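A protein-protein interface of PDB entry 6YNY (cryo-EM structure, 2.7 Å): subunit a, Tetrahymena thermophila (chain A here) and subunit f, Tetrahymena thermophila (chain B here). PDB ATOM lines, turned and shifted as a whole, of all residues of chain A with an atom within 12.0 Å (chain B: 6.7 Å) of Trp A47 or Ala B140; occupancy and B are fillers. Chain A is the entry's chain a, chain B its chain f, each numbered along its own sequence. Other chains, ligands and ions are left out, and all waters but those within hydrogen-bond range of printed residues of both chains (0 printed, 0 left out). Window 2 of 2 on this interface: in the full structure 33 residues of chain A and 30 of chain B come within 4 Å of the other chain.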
ATOM      1  N   GLY A  43     -17.058   6.937  11.977  1.00  0.00           N
ATOM      2  CA  GLY A  43     -15.899   7.413  12.694  1.00  0.00           C
ATOM      3  C   GLY A  43     -14.635   6.908  12.041  1.00  0.00           C
ATOM      4  O   GLY A  43     -14.232   5.759  12.237  1.00  0.00           O
ATOM      5  N   GLY A  44     -14.001   7.769  11.271  1.00  0.00           N
ATOM      6  CA  GLY A  44     -12.895   7.372  10.412  1.00  0.00           C
ATOM      7  C   GLY A  44     -11.937   8.508  10.230  1.00  0.00           C
ATOM      8  O   GLY A  44     -11.601   9.211  11.192  1.00  0.00           O
ATOM      9  N   VAL A  45     -11.500   8.712   8.994  1.00  0.00           N
ATOM     10  CA  VAL A  45     -10.509   9.725   8.666  1.00  0.00           C
ATOM     11  C   VAL A  45     -11.119  10.747   7.722  1.00  0.00           C
ATOM     12  O   VAL A  45     -11.992  10.430   6.908  1.00  0.00           O
ATOM     13  CB  VAL A  45      -9.243   9.098   8.053  1.00  0.00           C
ATOM     14  CG1 VAL A  45      -8.515   8.308   9.101  1.00  0.00           C
ATOM     15  CG2 VAL A  45      -9.603   8.211   6.883  1.00  0.00           C
ATOM     16  N   GLU A  46     -10.653  11.983   7.841  1.00  0.00           N
ATOM     17  CA  GLU A  46     -11.068  13.067   6.974  1.00  0.00           C
ATOM     18  C   GLU A  46     -10.008  13.285   5.898  1.00  0.00           C
ATOM     19  O   GLU A  46      -9.031  12.538   5.794  1.00  0.00           O
ATOM     20  CB  GLU A  46     -11.307  14.331   7.799  1.00  0.00           C
ATOM     21  CG  GLU A  46     -12.462  14.227   8.766  1.00  0.00           C
ATOM     22  CD  GLU A  46     -13.807  14.295   8.075  1.00  0.00           C
ATOM     23  OE1 GLU A  46     -13.843  14.197   6.832  1.00  0.00           O
ATOM     24  OE2 GLU A  46     -14.828  14.454   8.776  1.00  0.00           O
ATOM     25  N   TRP A  47     -10.191  14.326   5.087  1.00  0.00           N
ATOM     26  CA  TRP A  47      -9.235  14.610   4.026  1.00  0.00           C
ATOM     27  C   TRP A  47      -8.009  15.341   4.561  1.00  0.00           C
ATOM     28  O   TRP A  47      -6.874  14.935   4.298  1.00  0.00           O
ATOM     29  CB  TRP A  47      -9.906  15.423   2.919  1.00  0.00           C
ATOM     30  CG  TRP A  47      -8.957  15.834   1.858  1.00  0.00           C
ATOM     31  CD1 TRP A  47      -8.171  15.018   1.110  1.00  0.00           C
ATOM     32  CD2 TRP A  47      -8.688  17.165   1.418  1.00  0.00           C
ATOM     33  NE1 TRP A  47      -7.423  15.756   0.234  1.00  0.00           N
ATOM     34  CE2 TRP A  47      -7.724  17.080   0.402  1.00  0.00           C
ATOM     35  CE3 TRP A  47      -9.168  18.421   1.787  1.00  0.00           C
ATOM     36  CZ2 TRP A  47      -7.231  18.201  -0.250  1.00  0.00           C
ATOM     37  CZ3 TRP A  47      -8.677  19.531   1.141  1.00  0.00           C
ATOM     38  CH2 TRP A  47      -7.721  19.415   0.134  1.00  0.00           C
ATOM     39  N   VAL A  48      -8.222  16.420   5.307  1.00  0.00           N
ATOM     40  CA  VAL A  48      -7.139  17.223   5.858  1.00  0.00           C
ATOM     41  C   VAL A  48      -7.296  17.313   7.366  1.00  0.00           C
ATOM     42  O   VAL A  48      -8.405  17.275   7.905  1.00  0.00           O
ATOM     43  CB  VAL A  48      -7.088  18.640   5.249  1.00  0.00           C
ATOM     44  CG1 VAL A  48      -6.423  18.608   3.911  1.00  0.00           C
ATOM     45  CG2 VAL A  48      -8.474  19.214   5.133  1.00  0.00           C
ATOM     46  N   TYR A  49      -6.161  17.436   8.043  1.00  0.00           N
ATOM     47  CA  TYR A  49      -6.116  17.661   9.473  1.00  0.00           C
ATOM     48  C   TYR A  49      -5.179  18.823   9.762  1.00  0.00           C
ATOM     49  O   TYR A  49      -4.312  19.169   8.957  1.00  0.00           O
ATOM     50  CB  TYR A  49      -5.659  16.414  10.232  1.00  0.00           C
ATOM     51  CG  TYR A  49      -6.689  15.314  10.298  1.00  0.00           C
ATOM     52  CD1 TYR A  49      -6.501  14.119   9.628  1.00  0.00           C
ATOM     53  CD2 TYR A  49      -7.849  15.472  11.035  1.00  0.00           C
ATOM     54  CE1 TYR A  49      -7.438  13.113   9.690  1.00  0.00           C
ATOM     55  CE2 TYR A  49      -8.790  14.474  11.102  1.00  0.00           C
ATOM     56  CZ  TYR A  49      -8.581  13.296  10.427  1.00  0.00           C
ATOM     57  OH  TYR A  49      -9.521  12.299  10.494  1.00  0.00           O
ATOM     58  N   THR A  50      -5.370  19.420  10.930  1.00  0.00           N
ATOM     59  CA  THR A  50      -4.618  20.592  11.344  1.00  0.00           C
ATOM     60  C   THR A  50      -3.374  20.184  12.121  1.00  0.00           C
ATOM     61  O   THR A  50      -3.392  19.211  12.880  1.00  0.00           O
ATOM     62  CB  THR A  50      -5.504  21.505  12.191  1.00  0.00           C
ATOM     63  OG1 THR A  50      -6.393  22.230  11.334  1.00  0.00           O
ATOM     64  CG2 THR A  50      -4.677  22.478  13.012  1.00  0.00           C
ATOM     65  N   THR A  51      -2.294  20.934  11.922  1.00  0.00           N
ATOM     66  CA  THR A  51      -1.033  20.696  12.603  1.00  0.00           C
ATOM     67  C   THR A  51      -0.643  21.916  13.425  1.00  0.00           C
ATOM     68  O   THR A  51      -1.131  23.027  13.204  1.00  0.00           O
ATOM     69  CB  THR A  51       0.089  20.370  11.609  1.00  0.00           C
ATOM     70  OG1 THR A  51       0.267  21.462  10.701  1.00  0.00           O
ATOM     71  CG2 THR A  51      -0.230  19.117  10.830  1.00  0.00           C
ATOM     72  N   GLU A 158     -12.019  17.653 -16.071  1.00  0.00           N
ATOM     73  CA  GLU A 158     -12.804  18.469 -15.157  1.00  0.00           C
ATOM     74  C   GLU A 158     -12.461  19.940 -15.336  1.00  0.00           C
ATOM     75  O   GLU A 158     -11.289  20.304 -15.474  1.00  0.00           O
ATOM     76  CB  GLU A 158     -12.551  18.051 -13.708  1.00  0.00           C
ATOM     77  CG  GLU A 158     -12.859  16.594 -13.425  1.00  0.00           C
ATOM     78  CD  GLU A 158     -12.507  16.182 -12.009  1.00  0.00           C
ATOM     79  OE1 GLU A 158     -11.768  16.929 -11.336  1.00  0.00           O
ATOM     80  OE2 GLU A 158     -12.970  15.108 -11.569  1.00  0.00           O
ATOM     81  N   PHE A 159     -13.490  20.780 -15.328  1.00  0.00           N
ATOM     82  CA  PHE A 159     -13.312  22.218 -15.464  1.00  0.00           C
ATOM     83  C   PHE A 159     -13.005  22.830 -14.105  1.00  0.00           C
ATOM     84  O   PHE A 159     -13.777  22.668 -13.156  1.00  0.00           O
ATOM     85  CB  PHE A 159     -14.556  22.857 -16.066  1.00  0.00           C
ATOM     86  CG  PHE A 159     -14.705  22.623 -17.531  1.00  0.00           C
ATOM     87  CD1 PHE A 159     -14.126  23.483 -18.440  1.00  0.00           C
ATOM     88  CD2 PHE A 159     -15.430  21.550 -18.003  1.00  0.00           C
ATOM     89  CE1 PHE A 159     -14.263  23.275 -19.785  1.00  0.00           C
ATOM     90  CE2 PHE A 159     -15.568  21.340 -19.350  1.00  0.00           C
ATOM     91  CZ  PHE A 159     -14.983  22.204 -20.241  1.00  0.00           C
ATOM     92  N   VAL A 160     -11.877  23.528 -14.014  1.00  0.00           N
ATOM     93  CA  VAL A 160     -11.494  24.256 -12.816  1.00  0.00           C
ATOM     94  C   VAL A 160     -11.011  25.636 -13.231  1.00  0.00           C
ATOM     95  O   VAL A 160     -10.682  25.882 -14.393  1.00  0.00           O
ATOM     96  CB  VAL A 160     -10.401  23.528 -12.009  1.00  0.00           C
ATOM     97  CG1 VAL A 160     -10.840  22.129 -11.661  1.00  0.00           C
ATOM     98  CG2 VAL A 160      -9.109  23.499 -12.781  1.00  0.00           C
ATOM     99  N   TYR A 161     -10.973  26.541 -12.261  1.00  0.00           N
ATOM    100  CA  TYR A 161     -10.463  27.884 -12.484  1.00  0.00           C
ATOM    101  C   TYR A 161      -8.981  27.906 -12.132  1.00  0.00           C
ATOM    102  O   TYR A 161      -8.595  27.565 -11.010  1.00  0.00           O
ATOM    103  CB  TYR A 161     -11.245  28.909 -11.667  1.00  0.00           C
ATOM    104  CG  TYR A 161     -12.695  29.026 -12.069  1.00  0.00           C
ATOM    105  CD1 TYR A 161     -13.049  29.467 -13.331  1.00  0.00           C
ATOM    106  CD2 TYR A 161     -13.710  28.700 -11.187  1.00  0.00           C
ATOM    107  CE1 TYR A 161     -14.364  29.573 -13.702  1.00  0.00           C
ATOM    108  CE2 TYR A 161     -15.027  28.805 -11.553  1.00  0.00           C
ATOM    109  CZ  TYR A 161     -15.350  29.243 -12.810  1.00  0.00           C
ATOM    110  OH  TYR A 161     -16.669  29.349 -13.178  1.00  0.00           O
ATOM    111  N   PHE A 162      -8.158  28.292 -13.100  1.00  0.00           N
ATOM    112  CA  PHE A 162      -6.707  28.239 -12.981  1.00  0.00           C
ATOM    113  C   PHE A 162      -6.204  29.562 -12.417  1.00  0.00           C
ATOM    114  O   PHE A 162      -6.287  30.600 -13.080  1.00  0.00           O
ATOM    115  CB  PHE A 162      -6.096  27.939 -14.345  1.00  0.00           C
ATOM    116  CG  PHE A 162      -4.606  27.841 -14.346  1.00  0.00           C
ATOM    117  CD1 PHE A 162      -3.840  28.846 -14.896  1.00  0.00           C
ATOM    118  CD2 PHE A 162      -3.970  26.739 -13.820  1.00  0.00           C
ATOM    119  CE1 PHE A 162      -2.473  28.757 -14.912  1.00  0.00           C
ATOM    120  CE2 PHE A 162      -2.601  26.646 -13.834  1.00  0.00           C
ATOM    121  CZ  PHE A 162      -1.853  27.656 -14.380  1.00  0.00           C
ATOM    122  N   ASP A 163      -5.685  29.524 -11.196  1.00  0.00           N
ATOM    123  CA  ASP A 163      -5.223  30.726 -10.517  1.00  0.00           C
ATOM    124  C   ASP A 163      -3.884  31.166 -11.094  1.00  0.00           C
ATOM    125  O   ASP A 163      -2.891  30.438 -11.000  1.00  0.00           O
ATOM    126  CB  ASP A 163      -5.109  30.469  -9.018  1.00  0.00           C
ATOM    127  CG  ASP A 163      -4.886  31.733  -8.221  1.00  0.00           C
ATOM    128  OD1 ASP A 163      -4.740  32.810  -8.834  1.00  0.00           O
ATOM    129  OD2 ASP A 163      -4.861  31.651  -6.976  1.00  0.00           O
ATOM    130  N   LYS B 133      -8.056  25.122   7.132  1.00  0.00           N
ATOM    131  CA  LYS B 133      -8.537  23.825   6.673  1.00  0.00           C
ATOM    132  C   LYS B 133      -9.848  23.964   5.912  1.00  0.00           C
ATOM    133  O   LYS B 133     -10.086  23.242   4.939  1.00  0.00           O
ATOM    134  CB  LYS B 133      -8.691  22.884   7.865  1.00  0.00           C
ATOM    135  CG  LYS B 133      -9.603  21.694   7.646  1.00  0.00           C
ATOM    136  CD  LYS B 133      -9.611  20.794   8.860  1.00  0.00           C
ATOM    137  CE  LYS B 133     -10.522  19.603   8.671  1.00  0.00           C
ATOM    138  NZ  LYS B 133     -10.455  18.666   9.824  1.00  0.00           N
ATOM    139  N   TYR B 135     -10.717  26.705   4.270  1.00  0.00           N
ATOM    140  CA  TYR B 135     -10.387  27.381   3.023  1.00  0.00           C
ATOM    141  C   TYR B 135      -9.793  26.412   2.012  1.00  0.00           C
ATOM    142  O   TYR B 135     -10.112  26.476   0.820  1.00  0.00           O
ATOM    143  CB  TYR B 135      -9.423  28.531   3.293  1.00  0.00           C
ATOM    144  CG  TYR B 135      -9.016  29.270   2.050  1.00  0.00           C
ATOM    145  CD1 TYR B 135      -9.883  30.154   1.433  1.00  0.00           C
ATOM    146  CD2 TYR B 135      -7.764  29.088   1.495  1.00  0.00           C
ATOM    147  CE1 TYR B 135      -9.518  30.829   0.302  1.00  0.00           C
ATOM    148  CE2 TYR B 135      -7.390  29.758   0.363  1.00  0.00           C
ATOM    149  CZ  TYR B 135      -8.270  30.629  -0.232  1.00  0.00           C
ATOM    150  OH  TYR B 135      -7.896  31.303  -1.365  1.00  0.00           O
ATOM    151  N   ALA B 136      -8.927  25.508   2.467  1.00  0.00           N
ATOM    152  CA  ALA B 136      -8.406  24.478   1.579  1.00  0.00           C
ATOM    153  C   ALA B 136      -9.516  23.548   1.114  1.00  0.00           C
ATOM    154  O   ALA B 136      -9.520  23.098  -0.036  1.00  0.00           O
ATOM    155  CB  ALA B 136      -7.303  23.690   2.280  1.00  0.00           C
ATOM    156  N   THR B 137     -10.469  23.252   1.998  1.00  0.00           N
ATOM    157  CA  THR B 137     -11.612  22.440   1.608  1.00  0.00           C
ATOM    158  C   THR B 137     -12.492  23.169   0.605  1.00  0.00           C
ATOM    159  O   THR B 137     -13.076  22.537  -0.282  1.00  0.00           O
ATOM    160  CB  THR B 137     -12.419  22.051   2.846  1.00  0.00           C
ATOM    161  OG1 THR B 137     -11.648  21.171   3.669  1.00  0.00           O
ATOM    162  CG2 THR B 137     -13.694  21.372   2.458  1.00  0.00           C
ATOM    163  N   LEU B 138     -12.604  24.490   0.732  1.00  0.00           N
ATOM    164  CA  LEU B 138     -13.361  25.273  -0.236  1.00  0.00           C
ATOM    165  C   LEU B 138     -12.671  25.284  -1.593  1.00  0.00           C
ATOM    166  O   LEU B 138     -13.315  25.097  -2.631  1.00  0.00           O
ATOM    167  CB  LEU B 138     -13.542  26.693   0.291  1.00  0.00           C
ATOM    168  CG  LEU B 138     -14.436  27.635  -0.503  1.00  0.00           C
ATOM    169  CD1 LEU B 138     -15.864  27.152  -0.506  1.00  0.00           C
ATOM    170  CD2 LEU B 138     -14.334  29.018   0.079  1.00  0.00           C
ATOM    171  N   ARG B 139     -11.356  25.505  -1.605  1.00  0.00           N
ATOM    172  CA  ARG B 139     -10.609  25.478  -2.856  1.00  0.00           C
ATOM    173  C   ARG B 139     -10.632  24.098  -3.492  1.00  0.00           C
ATOM    174  O   ARG B 139     -10.543  23.979  -4.719  1.00  0.00           O
ATOM    175  CB  ARG B 139      -9.168  25.912  -2.609  1.00  0.00           C
ATOM    176  CG  ARG B 139      -9.021  27.325  -2.107  1.00  0.00           C
ATOM    177  CD  ARG B 139      -8.757  28.299  -3.222  1.00  0.00           C
ATOM    178  NE  ARG B 139      -7.475  28.056  -3.868  1.00  0.00           N
ATOM    179  CZ  ARG B 139      -6.842  28.945  -4.623  1.00  0.00           C
ATOM    180  NH1 ARG B 139      -7.363  30.145  -4.824  1.00  0.00           N
ATOM    181  NH2 ARG B 139      -5.680  28.634  -5.171  1.00  0.00           N
ATOM    182  N   ALA B 140     -10.741  23.049  -2.682  1.00  0.00           N
ATOM    183  CA  ALA B 140     -10.749  21.684  -3.185  1.00  0.00           C
ATOM    184  C   ALA B 140     -12.070  21.298  -3.835  1.00  0.00           C
ATOM    185  O   ALA B 140     -12.156  20.214  -4.419  1.00  0.00           O
ATOM    186  CB  ALA B 140     -10.429  20.710  -2.055  1.00  0.00           C
ATOM    187  N   GLY B 141     -13.087  22.139  -3.742  1.00  0.00           N
ATOM    188  CA  GLY B 141     -14.347  21.918  -4.404  1.00  0.00           C
ATOM    189  C   GLY B 141     -15.531  21.605  -3.520  1.00  0.00           C
ATOM    190  O   GLY B 141     -16.508  21.034  -4.015  1.00  0.00           O
ATOM    191  N   LYS B 142     -15.485  21.958  -2.241  1.00  0.00           N
ATOM    192  CA  LYS B 142     -16.582  21.714  -1.313  1.00  0.00           C
ATOM    193  C   LYS B 142     -17.051  23.050  -0.757  1.00  0.00           C
ATOM    194  O   LYS B 142     -16.356  23.667   0.058  1.00  0.00           O
ATOM    195  CB  LYS B 142     -16.145  20.782  -0.190  1.00  0.00           C
ATOM    196  CG  LYS B 142     -17.278  20.290   0.664  1.00  0.00           C
ATOM    197  CD  LYS B 142     -16.765  19.590   1.895  1.00  0.00           C
ATOM    198  CE  LYS B 142     -17.901  19.046   2.725  1.00  0.00           C
ATOM    199  NZ  LYS B 142     -18.909  20.089   3.022  1.00  0.00           N
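The side-chain amino group (NZ) of Lys B133 is in hydrogen-bond range of the backbone carbonyl oxygen (O) of Val A48, at 3.1 Å.
OD2 of Asp A163 is in salt-bridge range of NH2 of Arg B139 (3.6 Å).
O of Lys B133 sits at hydrogen-bond distance from OG1 of Thr B137.
O of Ala B136 touches CZ3 of Trp A47 (3.8 Å).
CH2 of Trp A47 touches CB of Ala B140, at 3.7 Å.
Trp A47 touches just these residues of chain B: Ala B136 and Ala B140.
Of the printed residues of chain B, Val A48 touches Lys B133 (3.1 Å).
Glu A158 touches none of the printed residues of chain B.
Phe A159 touches none of the printed residues of chain B.
Printed residues of chain B within 4 Å of Asp A163: Arg B139 (3.6 Å).
No residue of chain A comes within 4 Å of Leu B138.
Of chain A, only Trp A47 (3.7 Å) comes within 4 Å of Ala B140.
No residue of chain A comes within 4 Å of Gly B141.
The nearest residue of chain B that does not touch Trp A47 is Thr B137 (4.2 Å).
The nearest residue of chain A that does not touch Ala B140 is Val A48 (7.5 Å).
The nearest printed residue of chain A that does not touch Arg B139 is Trp A47 (6.6 Å).
Of the 15 printed residues of chain A, 3 touch a printed residue of chain B.
Of the 9 printed residues of chain B, 4 touch a printed residue of chain A.
Among the printed residues, 4 pairs touch across the chains.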
